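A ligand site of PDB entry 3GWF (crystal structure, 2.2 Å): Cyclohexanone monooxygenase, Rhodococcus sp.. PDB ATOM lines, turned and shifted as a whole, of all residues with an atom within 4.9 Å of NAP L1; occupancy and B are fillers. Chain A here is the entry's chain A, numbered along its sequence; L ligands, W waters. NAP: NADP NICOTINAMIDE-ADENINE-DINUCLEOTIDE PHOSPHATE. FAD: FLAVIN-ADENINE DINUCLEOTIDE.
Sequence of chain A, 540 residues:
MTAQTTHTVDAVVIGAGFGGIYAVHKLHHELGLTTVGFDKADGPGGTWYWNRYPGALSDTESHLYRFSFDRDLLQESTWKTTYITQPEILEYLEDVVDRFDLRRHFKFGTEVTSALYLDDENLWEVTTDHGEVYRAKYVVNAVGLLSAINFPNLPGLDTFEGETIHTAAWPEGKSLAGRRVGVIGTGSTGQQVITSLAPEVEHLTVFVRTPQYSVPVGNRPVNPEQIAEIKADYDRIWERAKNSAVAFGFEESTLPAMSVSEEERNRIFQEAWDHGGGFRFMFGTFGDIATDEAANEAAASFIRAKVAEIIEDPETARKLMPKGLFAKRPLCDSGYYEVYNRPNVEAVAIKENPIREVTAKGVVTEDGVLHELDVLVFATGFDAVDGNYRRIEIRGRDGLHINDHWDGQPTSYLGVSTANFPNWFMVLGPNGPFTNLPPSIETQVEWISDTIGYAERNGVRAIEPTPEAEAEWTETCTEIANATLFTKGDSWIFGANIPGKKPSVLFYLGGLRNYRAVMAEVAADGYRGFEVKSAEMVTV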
ATOM      1  N   TYR A  53      19.557  10.513 -14.325  1.00  0.00           N
ATOM      2  CA  TYR A  53      18.286  10.407 -15.033  1.00  0.00           C
ATOM      3  C   TYR A  53      17.282  11.469 -14.565  1.00  0.00           C
ATOM      4  O   TYR A  53      17.381  11.950 -13.436  1.00  0.00           O
ATOM      5  CB  TYR A  53      17.711   8.996 -14.910  1.00  0.00           C
ATOM      6  CG  TYR A  53      17.375   8.553 -13.500  1.00  0.00           C
ATOM      7  CD1 TYR A  53      16.150   8.858 -12.928  1.00  0.00           C
ATOM      8  CD2 TYR A  53      18.290   7.815 -12.748  1.00  0.00           C
ATOM      9  CE1 TYR A  53      15.812   8.438 -11.653  1.00  0.00           C
ATOM     10  CE2 TYR A  53      17.979   7.403 -11.464  1.00  0.00           C
ATOM     11  CZ  TYR A  53      16.732   7.719 -10.925  1.00  0.00           C
ATOM     12  OH  TYR A  53      16.424   7.303  -9.669  1.00  0.00           O
ATOM     13  N   LEU A  57      15.507  11.560  -7.450  1.00  0.00           N
ATOM     14  CA  LEU A  57      15.111  12.234  -6.251  1.00  0.00           C
ATOM     15  C   LEU A  57      15.362  11.317  -5.060  1.00  0.00           C
ATOM     16  O   LEU A  57      15.189  10.109  -5.159  1.00  0.00           O
ATOM     17  CB  LEU A  57      13.622  12.602  -6.324  1.00  0.00           C
ATOM     18  CG  LEU A  57      13.055  13.555  -5.254  1.00  0.00           C
ATOM     19  CD1 LEU A  57      13.329  15.012  -5.655  1.00  0.00           C
ATOM     20  CD2 LEU A  57      11.569  13.354  -5.032  1.00  0.00           C
ATOM     21  N   SER A  58      15.779  11.908  -3.931  1.00  0.00           N
ATOM     22  CA  SER A  58      15.947  11.176  -2.674  1.00  0.00           C
ATOM     23  C   SER A  58      14.617  10.659  -2.102  1.00  0.00           C
ATOM     24  O   SER A  58      13.548  11.165  -2.442  1.00  0.00           O
ATOM     25  CB  SER A  58      16.633  12.090  -1.654  1.00  0.00           C
ATOM     26  OG  SER A  58      15.763  13.102  -1.175  1.00  0.00           O
ATOM     27  N   ASP A  59      14.660   9.650  -1.232  1.00  0.00           N
ATOM     28  CA  ASP A  59      13.480   9.274  -0.477  1.00  0.00           C
ATOM     29  C   ASP A  59      13.605   9.670   0.988  1.00  0.00           C
ATOM     30  O   ASP A  59      12.698   9.445   1.781  1.00  0.00           O
ATOM     31  CB  ASP A  59      13.084   7.794  -0.688  1.00  0.00           C
ATOM     32  CG  ASP A  59      14.090   6.806  -0.105  1.00  0.00           C
ATOM     33  OD1 ASP A  59      15.063   7.197   0.573  1.00  0.00           O
ATOM     34  OD2 ASP A  59      13.911   5.598  -0.328  1.00  0.00           O
ATOM     35  N   ASN A 150      22.763  -3.882 -15.301  1.00  0.00           N
ATOM     36  CA  ASN A 150      21.861  -4.940 -15.824  1.00  0.00           C
ATOM     37  C   ASN A 150      21.085  -4.451 -17.051  1.00  0.00           C
ATOM     38  O   ASN A 150      20.100  -3.702 -16.917  1.00  0.00           O
ATOM     39  CB  ASN A 150      20.932  -5.502 -14.737  1.00  0.00           C
ATOM     40  CG  ASN A 150      19.831  -6.428 -15.287  1.00  0.00           C
ATOM     41  OD1 ASN A 150      18.774  -6.576 -14.672  1.00  0.00           O
ATOM     42  ND2 ASN A 150      20.087  -7.059 -16.439  1.00  0.00           N
ATOM     43  N   PRO A 152      19.320  -5.867 -20.168  1.00  0.00           N
ATOM     44  CA  PRO A 152      18.776  -7.187 -20.555  1.00  0.00           C
ATOM     45  C   PRO A 152      18.903  -7.566 -22.028  1.00  0.00           C
ATOM     46  O   PRO A 152      18.991  -6.716 -22.904  1.00  0.00           O
ATOM     47  CB  PRO A 152      17.296  -7.115 -20.156  1.00  0.00           C
ATOM     48  CG  PRO A 152      17.004  -5.683 -19.988  1.00  0.00           C
ATOM     49  CD  PRO A 152      18.282  -5.058 -19.494  1.00  0.00           C
ATOM     50  N   THR A 167      19.334   4.058 -17.325  1.00  0.00           N
ATOM     51  CA  THR A 167      19.214   5.171 -16.370  1.00  0.00           C
ATOM     52  C   THR A 167      20.509   5.492 -15.618  1.00  0.00           C
ATOM     53  O   THR A 167      20.736   6.627 -15.223  1.00  0.00           O
ATOM     54  CB  THR A 167      18.075   4.919 -15.364  1.00  0.00           C
ATOM     55  OG1 THR A 167      18.292   3.663 -14.704  1.00  0.00           O
ATOM     56  CG2 THR A 167      16.727   4.861 -16.076  1.00  0.00           C
ATOM     57  N   ILE A 184      11.530   0.176 -19.788  1.00  0.00           N
ATOM     58  CA  ILE A 184      11.467  -1.152 -19.187  1.00  0.00           C
ATOM     59  C   ILE A 184      11.990  -1.077 -17.759  1.00  0.00           C
ATOM     60  O   ILE A 184      13.146  -0.704 -17.554  1.00  0.00           O
ATOM     61  CB  ILE A 184      12.323  -2.167 -19.971  1.00  0.00           C
ATOM     62  CG1 ILE A 184      11.786  -2.300 -21.391  1.00  0.00           C
ATOM     63  CG2 ILE A 184      12.318  -3.528 -19.249  1.00  0.00           C
ATOM     64  CD1 ILE A 184      12.725  -3.006 -22.341  1.00  0.00           C
ATOM     65  N   GLY A 185      11.138  -1.421 -16.794  1.00  0.00           N
ATOM     66  CA  GLY A 185      11.512  -1.396 -15.369  1.00  0.00           C
ATOM     67  C   GLY A 185      10.684  -0.435 -14.536  1.00  0.00           C
ATOM     68  O   GLY A 185      10.533   0.747 -14.907  1.00  0.00           O
ATOM     69  N   THR A 186      10.123  -0.917 -13.438  1.00  0.00           N
ATOM     70  CA  THR A 186       9.242  -0.098 -12.594  1.00  0.00           C
ATOM     71  C   THR A 186       9.634  -0.136 -11.105  1.00  0.00           C
ATOM     72  O   THR A 186       8.784  -0.053 -10.215  1.00  0.00           O
ATOM     73  CB  THR A 186       7.735  -0.466 -12.772  1.00  0.00           C
ATOM     74  OG1 THR A 186       7.517  -1.845 -12.406  1.00  0.00           O
ATOM     75  CG2 THR A 186       7.269  -0.244 -14.231  1.00  0.00           C
ATOM     76  N   GLY A 187      10.942  -0.238 -10.841  1.00  0.00           N
ATOM     77  CA  GLY A 187      11.465  -0.022  -9.510  1.00  0.00           C
ATOM     78  C   GLY A 187      11.408   1.461  -9.191  1.00  0.00           C
ATOM     79  O   GLY A 187      10.742   2.232  -9.902  1.00  0.00           O
ATOM     80  N   SER A 188      12.110   1.882  -8.140  1.00  0.00           N
ATOM     81  CA  SER A 188      12.153   3.299  -7.761  1.00  0.00           C
ATOM     82  C   SER A 188      12.627   4.164  -8.923  1.00  0.00           C
ATOM     83  O   SER A 188      12.011   5.167  -9.242  1.00  0.00           O
ATOM     84  CB  SER A 188      13.055   3.500  -6.553  1.00  0.00           C
ATOM     85  OG  SER A 188      14.157   2.636  -6.673  1.00  0.00           O
ATOM     86  N   THR A 189      13.700   3.727  -9.592  1.00  0.00           N
ATOM     87  CA  THR A 189      14.271   4.478 -10.700  1.00  0.00           C
ATOM     88  C   THR A 189      13.300   4.625 -11.877  1.00  0.00           C
ATOM     89  O   THR A 189      13.095   5.729 -12.371  1.00  0.00           O
ATOM     90  CB  THR A 189      15.599   3.876 -11.156  1.00  0.00           C
ATOM     91  OG1 THR A 189      16.607   4.197 -10.194  1.00  0.00           O
ATOM     92  CG2 THR A 189      16.026   4.461 -12.485  1.00  0.00           C
ATOM     93  N   GLY A 190      12.708   3.507 -12.299  1.00  0.00           N
ATOM     94  CA  GLY A 190      11.770   3.513 -13.425  1.00  0.00           C
ATOM     95  C   GLY A 190      10.540   4.368 -13.189  1.00  0.00           C
ATOM     96  O   GLY A 190      10.143   5.119 -14.081  1.00  0.00           O
ATOM     97  N   ARG A 209       6.655  -5.454 -15.436  1.00  0.00           N
ATOM     98  CA  ARG A 209       6.756  -6.868 -15.096  1.00  0.00           C
ATOM     99  C   ARG A 209       6.142  -7.113 -13.721  1.00  0.00           C
ATOM    100  O   ARG A 209       5.274  -7.978 -13.578  1.00  0.00           O
ATOM    101  CB  ARG A 209       8.194  -7.377 -15.171  1.00  0.00           C
ATOM    102  CG  ARG A 209       8.281  -8.895 -15.400  1.00  0.00           C
ATOM    103  CD  ARG A 209       9.670  -9.339 -15.811  1.00  0.00           C
ATOM    104  NE  ARG A 209      10.657  -9.219 -14.723  1.00  0.00           N
ATOM    105  CZ  ARG A 209      11.940  -9.525 -14.831  1.00  0.00           C
ATOM    106  NH1 ARG A 209      12.434  -9.978 -15.977  1.00  0.00           N
ATOM    107  NH2 ARG A 209      12.746  -9.389 -13.790  1.00  0.00           N
ATOM    108  N   THR A 210       6.599  -6.351 -12.725  1.00  0.00           N
ATOM    109  CA  THR A 210       6.067  -6.448 -11.365  1.00  0.00           C
ATOM    110  C   THR A 210       5.727  -5.048 -10.872  1.00  0.00           C
ATOM    111  O   THR A 210       6.620  -4.249 -10.573  1.00  0.00           O
ATOM    112  CB  THR A 210       7.063  -7.141 -10.386  1.00  0.00           C
ATOM    113  OG1 THR A 210       7.760  -8.196 -11.053  1.00  0.00           O
ATOM    114  CG2 THR A 210       6.320  -7.735  -9.205  1.00  0.00           C
ATOM    115  N   GLN A 212       4.714  -2.299  -8.227  1.00  0.00           N
ATOM    116  CA  GLN A 212       5.162  -2.190  -6.851  1.00  0.00           C
ATOM    117  C   GLN A 212       4.242  -1.287  -6.084  1.00  0.00           C
ATOM    118  O   GLN A 212       3.538  -0.472  -6.671  1.00  0.00           O
ATOM    119  CB  GLN A 212       6.562  -1.590  -6.792  1.00  0.00           C
ATOM    120  CG  GLN A 212       7.576  -2.308  -7.637  1.00  0.00           C
ATOM    121  CD  GLN A 212       8.478  -3.173  -6.799  1.00  0.00           C
ATOM    122  OE1 GLN A 212       9.392  -2.671  -6.141  1.00  0.00           O
ATOM    123  NE2 GLN A 212       8.224  -4.481  -6.812  1.00  0.00           N
ATOM    124  N   ARG A 329      12.362  -1.712   1.044  1.00  0.00           N
ATOM    125  CA  ARG A 329      12.314  -0.247   0.970  1.00  0.00           C
ATOM    126  C   ARG A 329      11.048   0.195   0.239  1.00  0.00           C
ATOM    127  O   ARG A 329      10.848  -0.166  -0.917  1.00  0.00           O
ATOM    128  CB  ARG A 329      13.588   0.349   0.333  1.00  0.00           C
ATOM    129  CG  ARG A 329      13.680   1.872   0.476  1.00  0.00           C
ATOM    130  CD  ARG A 329      15.064   2.438   0.155  1.00  0.00           C
ATOM    131  NE  ARG A 329      15.997   2.386   1.289  1.00  0.00           N
ATOM    132  CZ  ARG A 329      16.494   3.450   1.925  1.00  0.00           C
ATOM    133  NH1 ARG A 329      16.162   4.688   1.558  1.00  0.00           N
ATOM    134  NH2 ARG A 329      17.350   3.268   2.942  1.00  0.00           N
ATOM    135  N   ILE A 350       4.002  -7.388 -19.314  1.00  0.00           N
ATOM    136  CA  ILE A 350       4.806  -8.344 -20.078  1.00  0.00           C
ATOM    137  C   ILE A 350       4.748  -9.776 -19.567  1.00  0.00           C
ATOM    138  O   ILE A 350       5.124 -10.693 -20.292  1.00  0.00           O
ATOM    139  CB  ILE A 350       6.275  -7.883 -20.319  1.00  0.00           C
ATOM    140  CG1 ILE A 350       7.007  -7.638 -18.988  1.00  0.00           C
ATOM    141  CG2 ILE A 350       6.310  -6.679 -21.271  1.00  0.00           C
ATOM    142  CD1 ILE A 350       8.517  -7.371 -19.139  1.00  0.00           C
ATOM    143  N   ALA A 379      15.309   0.891 -17.153  1.00  0.00           N
ATOM    144  CA  ALA A 379      15.367   1.214 -15.748  1.00  0.00           C
ATOM    145  C   ALA A 379      15.371  -0.138 -15.040  1.00  0.00           C
ATOM    146  O   ALA A 379      14.601  -0.405 -14.122  1.00  0.00           O
ATOM    147  CB  ALA A 379      14.161   2.067 -15.364  1.00  0.00           C
ATOM    148  N   THR A 380      16.276  -0.986 -15.500  1.00  0.00           N
ATOM    149  CA  THR A 380      16.287  -2.400 -15.135  1.00  0.00           C
ATOM    150  C   THR A 380      17.313  -2.706 -14.039  1.00  0.00           C
ATOM    151  O   THR A 380      17.625  -3.873 -13.758  1.00  0.00           O
ATOM    152  CB  THR A 380      16.465  -3.302 -16.401  1.00  0.00           C
ATOM    153  OG1 THR A 380      17.421  -2.713 -17.279  1.00  0.00           O
ATOM    154  CG2 THR A 380      15.162  -3.432 -17.130  1.00  0.00           C
ATOM    155  N   GLY A 381      17.833  -1.650 -13.420  1.00  0.00           N
ATOM    156  CA  GLY A 381      18.764  -1.769 -12.303  1.00  0.00           C
ATOM    157  C   GLY A 381      20.062  -2.460 -12.661  1.00  0.00           C
ATOM    158  O   GLY A 381      20.515  -2.410 -13.805  1.00  0.00           O
ATOM    159  N   PHE A 382      20.646  -3.118 -11.661  1.00  0.00           N
ATOM    160  CA  PHE A 382      21.971  -3.717 -11.741  1.00  0.00           C
ATOM    161  C   PHE A 382      21.924  -5.190 -11.330  1.00  0.00           C
ATOM    162  O   PHE A 382      20.910  -5.659 -10.813  1.00  0.00           O
ATOM    163  CB  PHE A 382      22.936  -2.970 -10.816  1.00  0.00           C
ATOM    164  CG  PHE A 382      22.926  -1.479 -10.984  1.00  0.00           C
ATOM    165  CD1 PHE A 382      22.011  -0.695 -10.291  1.00  0.00           C
ATOM    166  CD2 PHE A 382      23.843  -0.863 -11.829  1.00  0.00           C
ATOM    167  CE1 PHE A 382      21.990   0.701 -10.458  1.00  0.00           C
ATOM    168  CE2 PHE A 382      23.837   0.516 -11.999  1.00  0.00           C
ATOM    169  CZ  PHE A 382      22.905   1.310 -11.309  1.00  0.00           C
HETATM  170  PA  NAP L   1      15.369  -2.362  -9.528  1.00  0.00           P
HETATM  171  O1A NAP L   1      16.069  -3.665  -9.522  1.00  0.00           O
HETATM  172  O2A NAP L   1      14.835  -1.984  -8.201  1.00  0.00           O
HETATM  173  O5B NAP L   1      14.195  -2.440 -10.626  1.00  0.00           O
HETATM  174  C5B NAP L   1      14.392  -3.115 -11.843  1.00  0.00           C
HETATM  175  C4B NAP L   1      13.084  -3.096 -12.628  1.00  0.00           C
HETATM  176  O4B NAP L   1      13.316  -3.641 -13.914  1.00  0.00           O
HETATM  177  C3B NAP L   1      12.022  -3.968 -11.981  1.00  0.00           C
HETATM  178  O3B NAP L   1      10.748  -3.451 -12.335  1.00  0.00           O
HETATM  179  C2B NAP L   1      12.242  -5.286 -12.670  1.00  0.00           C
HETATM  180  O2B NAP L   1      11.079  -6.072 -12.594  1.00  0.00           O
HETATM  181  C1B NAP L   1      12.591  -4.844 -14.085  1.00  0.00           C
HETATM  182  N9A NAP L   1      13.417  -5.790 -14.870  1.00  0.00           N
HETATM  183  C8A NAP L   1      14.666  -6.276 -14.539  1.00  0.00           C
HETATM  184  N7A NAP L   1      15.075  -7.089 -15.538  1.00  0.00           N
HETATM  185  C5A NAP L   1      14.134  -7.125 -16.506  1.00  0.00           C
HETATM  186  C6A NAP L   1      14.052  -7.810 -17.727  1.00  0.00           C
HETATM  187  N6A NAP L   1      15.037  -8.602 -18.129  1.00  0.00           N
HETATM  188  N1A NAP L   1      12.935  -7.651 -18.506  1.00  0.00           N
HETATM  189  C2A NAP L   1      11.897  -6.840 -18.085  1.00  0.00           C
HETATM  190  N3A NAP L   1      11.986  -6.170 -16.882  1.00  0.00           N
HETATM  191  C4A NAP L   1      13.076  -6.312 -16.096  1.00  0.00           C
HETATM  192  O3  NAP L   1      16.351  -1.219 -10.146  1.00  0.00           O
HETATM  193  PN  NAP L   1      16.321   0.382  -9.895  1.00  0.00           P
HETATM  194  O1N NAP L   1      14.945   0.880  -9.709  1.00  0.00           O
HETATM  195  O2N NAP L   1      17.163   0.982 -10.971  1.00  0.00           O
HETATM  196  O5D NAP L   1      17.147   0.563  -8.519  1.00  0.00           O
HETATM  197  C5D NAP L   1      18.478   0.051  -8.448  1.00  0.00           C
HETATM  198  C4D NAP L   1      18.890  -0.274  -7.022  1.00  0.00           C
HETATM  199  O4D NAP L   1      19.165   0.934  -6.337  1.00  0.00           O
HETATM  200  C3D NAP L   1      17.829  -1.032  -6.235  1.00  0.00           C
HETATM  201  O3D NAP L   1      18.441  -2.147  -5.629  1.00  0.00           O
HETATM  202  C2D NAP L   1      17.320  -0.066  -5.174  1.00  0.00           C
HETATM  203  O2D NAP L   1      17.258  -0.661  -3.906  1.00  0.00           O
HETATM  204  C1D NAP L   1      18.331   1.081  -5.196  1.00  0.00           C
HETATM  205  N1N NAP L   1      17.652   2.395  -5.209  1.00  0.00           N
HETATM  206  C2N NAP L   1      17.425   3.028  -4.024  1.00  0.00           C
HETATM  207  C3N NAP L   1      16.791   4.265  -4.018  1.00  0.00           C
HETATM  208  C7N NAP L   1      16.552   4.941  -2.720  1.00  0.00           C
HETATM  209  O7N NAP L   1      15.598   5.981  -2.676  1.00  0.00           O
HETATM  210  N7N NAP L   1      17.244   4.550  -1.644  1.00  0.00           N
HETATM  211  C4N NAP L   1      16.386   4.868  -5.210  1.00  0.00           C
HETATM  212  C5N NAP L   1      16.633   4.220  -6.418  1.00  0.00           C
HETATM  213  C6N NAP L   1      17.269   2.975  -6.401  1.00  0.00           C
HETATM  214  P2B NAP L   1      11.001  -7.278 -11.510  1.00  0.00           P
HETATM  215  O1X NAP L   1      10.544  -6.698 -10.194  1.00  0.00           O
HETATM  216  O2X NAP L   1      10.058  -8.327 -12.039  1.00  0.00           O
HETATM  217  O3X NAP L   1      12.378  -7.867 -11.325  1.00  0.00           O
HETATM  218  PA  FAD L   2      28.219   5.097  -3.749  1.00  0.00           P
HETATM  219  O1A FAD L   2      27.465   4.080  -4.543  1.00  0.00           O
HETATM  220  O2A FAD L   2      27.553   6.447  -3.825  1.00  0.00           O
HETATM  221  O5B FAD L   2      29.746   5.302  -4.184  1.00  0.00           O
HETATM  222  C5B FAD L   2      30.586   4.198  -4.419  1.00  0.00           C
HETATM  223  C4B FAD L   2      31.648   4.600  -5.418  1.00  0.00           C
HETATM  224  O4B FAD L   2      32.621   3.584  -5.434  1.00  0.00           O
HETATM  225  C3B FAD L   2      31.116   4.722  -6.860  1.00  0.00           C
HETATM  226  O3B FAD L   2      31.269   6.047  -7.340  1.00  0.00           O
HETATM  227  C2B FAD L   2      31.982   3.775  -7.662  1.00  0.00           C
HETATM  228  O2B FAD L   2      32.393   4.329  -8.900  1.00  0.00           O
HETATM  229  C1B FAD L   2      33.180   3.554  -6.725  1.00  0.00           C
HETATM  230  N9A FAD L   2      33.841   2.264  -6.935  1.00  0.00           N
HETATM  231  C8A FAD L   2      33.294   1.004  -6.792  1.00  0.00           C
HETATM  232  N7A FAD L   2      34.250   0.106  -7.091  1.00  0.00           N
HETATM  233  C5A FAD L   2      35.397   0.770  -7.416  1.00  0.00           C
HETATM  234  C6A FAD L   2      36.659   0.342  -7.802  1.00  0.00           C
HETATM  235  N6A FAD L   2      36.923  -0.958  -7.917  1.00  0.00           N
HETATM  236  N1A FAD L   2      37.644   1.272  -8.071  1.00  0.00           N
HETATM  237  C2A FAD L   2      37.377   2.623  -7.966  1.00  0.00           C
HETATM  238  N3A FAD L   2      36.121   3.039  -7.584  1.00  0.00           N
HETATM  239  C4A FAD L   2      35.151   2.132  -7.317  1.00  0.00           C
HETATM  240  N1  FAD L   2      19.776   6.312   0.417  1.00  0.00           N
HETATM  241  C2  FAD L   2      19.171   6.946   1.488  1.00  0.00           C
HETATM  242  O2  FAD L   2      19.472   6.664   2.632  1.00  0.00           O
HETATM  243  N3  FAD L   2      18.210   7.899   1.285  1.00  0.00           N
HETATM  244  C4  FAD L   2      17.854   8.237   0.009  1.00  0.00           C
HETATM  245  O4  FAD L   2      16.998   9.093  -0.178  1.00  0.00           O
HETATM  246  C4X FAD L   2      18.442   7.604  -1.086  1.00  0.00           C
HETATM  247  N5  FAD L   2      18.067   7.954  -2.353  1.00  0.00           N
HETATM  248  C5X FAD L   2      18.665   7.340  -3.442  1.00  0.00           C
HETATM  249  C6  FAD L   2      18.260   7.717  -4.711  1.00  0.00           C
HETATM  250  C7  FAD L   2      18.820   7.124  -5.838  1.00  0.00           C
HETATM  251  C7M FAD L   2      18.358   7.571  -7.190  1.00  0.00           C
HETATM  252  C8  FAD L   2      19.812   6.162  -5.688  1.00  0.00           C
HETATM  253  C8M FAD L   2      20.435   5.505  -6.897  1.00  0.00           C
HETATM  254  C9  FAD L   2      20.222   5.785  -4.390  1.00  0.00           C
HETATM  255  C9A FAD L   2      19.662   6.378  -3.263  1.00  0.00           C
HETATM  256  N10 FAD L   2      20.050   6.023  -1.965  1.00  0.00           N
HETATM  257  C10 FAD L   2      19.432   6.640  -0.885  1.00  0.00           C
HETATM  258  C1' FAD L   2      21.122   5.005  -1.693  1.00  0.00           C
HETATM  259  C2' FAD L   2      22.522   5.618  -1.854  1.00  0.00           C
HETATM  260  O2' FAD L   2      23.319   4.682  -2.543  1.00  0.00           O
HETATM  261  C3' FAD L   2      23.187   6.046  -0.527  1.00  0.00           C
HETATM  262  O3' FAD L   2      22.371   6.968   0.155  1.00  0.00           O
HETATM  263  C4' FAD L   2      24.584   6.679  -0.677  1.00  0.00           C
HETATM  264  O4' FAD L   2      24.673   7.583  -1.772  1.00  0.00           O
HETATM  265  C5' FAD L   2      25.640   5.605  -0.839  1.00  0.00           C
HETATM  266  O5' FAD L   2      26.945   6.164  -0.785  1.00  0.00           O
HETATM  267  P   FAD L   2      28.195   5.169  -0.857  1.00  0.00           P
HETATM  268  O1P FAD L   2      29.440   6.001  -0.706  1.00  0.00           O
HETATM  269  O2P FAD L   2      28.074   4.096   0.191  1.00  0.00           O
HETATM  270  O3P FAD L   2      28.256   4.426  -2.281  1.00  0.00           O
HETATM  271  O   HOH W   1       8.185  -4.119 -13.666  1.00  0.00           O
HETATM  272  O   HOH W   2      13.484   0.746 -11.970  1.00  0.00           O
HETATM  273  O   HOH W   3      18.820   2.793 -10.397  1.00  0.00           O
HETATM  274  O   HOH W   4      17.845   1.070 -13.555  1.00  0.00           O
HETATM  275  O   HOH W   5      13.747  -0.150  -6.693  1.00  0.00           O
HETATM  276  O   HOH W   6      18.737   2.820  -0.174  1.00  0.00           O
HETATM  277  O   HOH W   7      19.299  -3.370  -9.205  1.00  0.00           O
HETATM  278  O   HOH W   8      13.948   2.946  -3.035  1.00  0.00           O
HETATM  279  O   HOH W   9       9.215  -4.300 -10.429  1.00  0.00           O
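Water W3 bridges an oxygen (O2N) of NAP L1 (2.5 Å) and the side-chain hydroxyl (OG1) of Thr 189 (2.6 Å).
Water W5 lies within hydrogen-bond range of O2A of NAP L1 (2.6 Å) and OG of Ser 188 (2.8 Å).
Water W4 lies within hydrogen-bond range of O2N of NAP L1, N of Gly 381, OG1 of Thr 167 and N of Thr 380.
Water W2 lies within hydrogen-bond range of the backbone carbonyl oxygen of Ala 379 (2.7 Å), an oxygen (O1N) of NAP L1 (2.7 Å), the backbone NH of Gly 190 (2.9 Å) and the backbone NH of Gly 187 (3.0 Å).
Water W1 lies within hydrogen-bond range of the side-chain hydroxyl (OG1) of Thr 186 (2.7 Å), the backbone NH (N) of Arg 209 (2.7 Å), the backbone NH (N) of Thr 210 (2.9 Å) and an oxygen (O3B) of NAP L1 (3.0 Å).
Water W7 bridges N of Phe 382 and O1A of NAP L1.
OG1 of Thr 189 sits close to O2N of NAP L1.
An oxygen (O1N) of NAP L1 sits at hydrogen-bond distance from the backbone NH (N) of Ser 188, at 3.4 Å.
OG1 of Thr 210 lies within hydrogen-bond range of O2X of NAP L1 (2.5 Å).
The backbone NH (N) of Thr 186 sits at hydrogen-bond distance from an oxygen (O3B) of NAP L1 (2.8 Å).
The guanidinium group of Arg 209 is in salt-bridge range of an oxygen (O2X) of NAP L1 (2.9 Å).
N3 of FAD L2 sits close to OD1 of Asp 59, 3.3 Å away.
An oxygen (O4) of FAD L2 lies within hydrogen-bond range of the backbone NH of Asp 59, at 2.6 Å.
An oxygen (O1N) of NAP L1 lies within hydrogen-bond range of the backbone NH (N) of Thr 189 (3.1 Å).
An oxygen (O7N) of NAP L1 lies close to the side-chain carboxylate (OD2) of Asp 59, at 2.9 Å.
A nitrogen (N7N) of NAP L1 lies close to the guanidinium group of Arg 329 (3.4 Å).
The backbone carbonyl oxygen (O) of Ala 379 sits close to an oxygen (O4B) of NAP L1 (3.5 Å).
Residues that only touch NAP L1: Gly 185, Gly 381, Pro 152, Thr 380, Ile 184, Gly 187, Ile 350 and Asn 150.
Within 4 Å of NAP L1: Asp 59, Asn 150, Pro 152, Ile 184, Gly 185, Thr 186, Gly 187, Ser 188, Thr 189, Arg 209, Thr 210, Arg 329, Ile 350, Ala 379, Thr 380 and Gly 381.
The nearest printed residue that does not touch NAP L1 is Phe 382 (4.1 Å).
N of Ala 379 lies within hydrogen-bond range of O of Ile 184.
The side-chain carboxylate (OD1) of Asp 59 is in salt-bridge range of the guanidinium group (NH1) of Arg 329, 2.9 Å away.
OG1 of Thr 380 lies within hydrogen-bond range of O of Asn 150 (2.9 Å).
O of Thr 210 is in hydrogen-bond range of OG1 of Thr 186 (3.2 Å).
The side-chain hydroxyl (OG1) of Thr 189 is in hydrogen-bond range of the side-chain hydroxyl (OH) of Tyr 53, 3.2 Å away.
O of Gly 381 lies within hydrogen-bond range of N of Asn 150 (3.1 Å).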
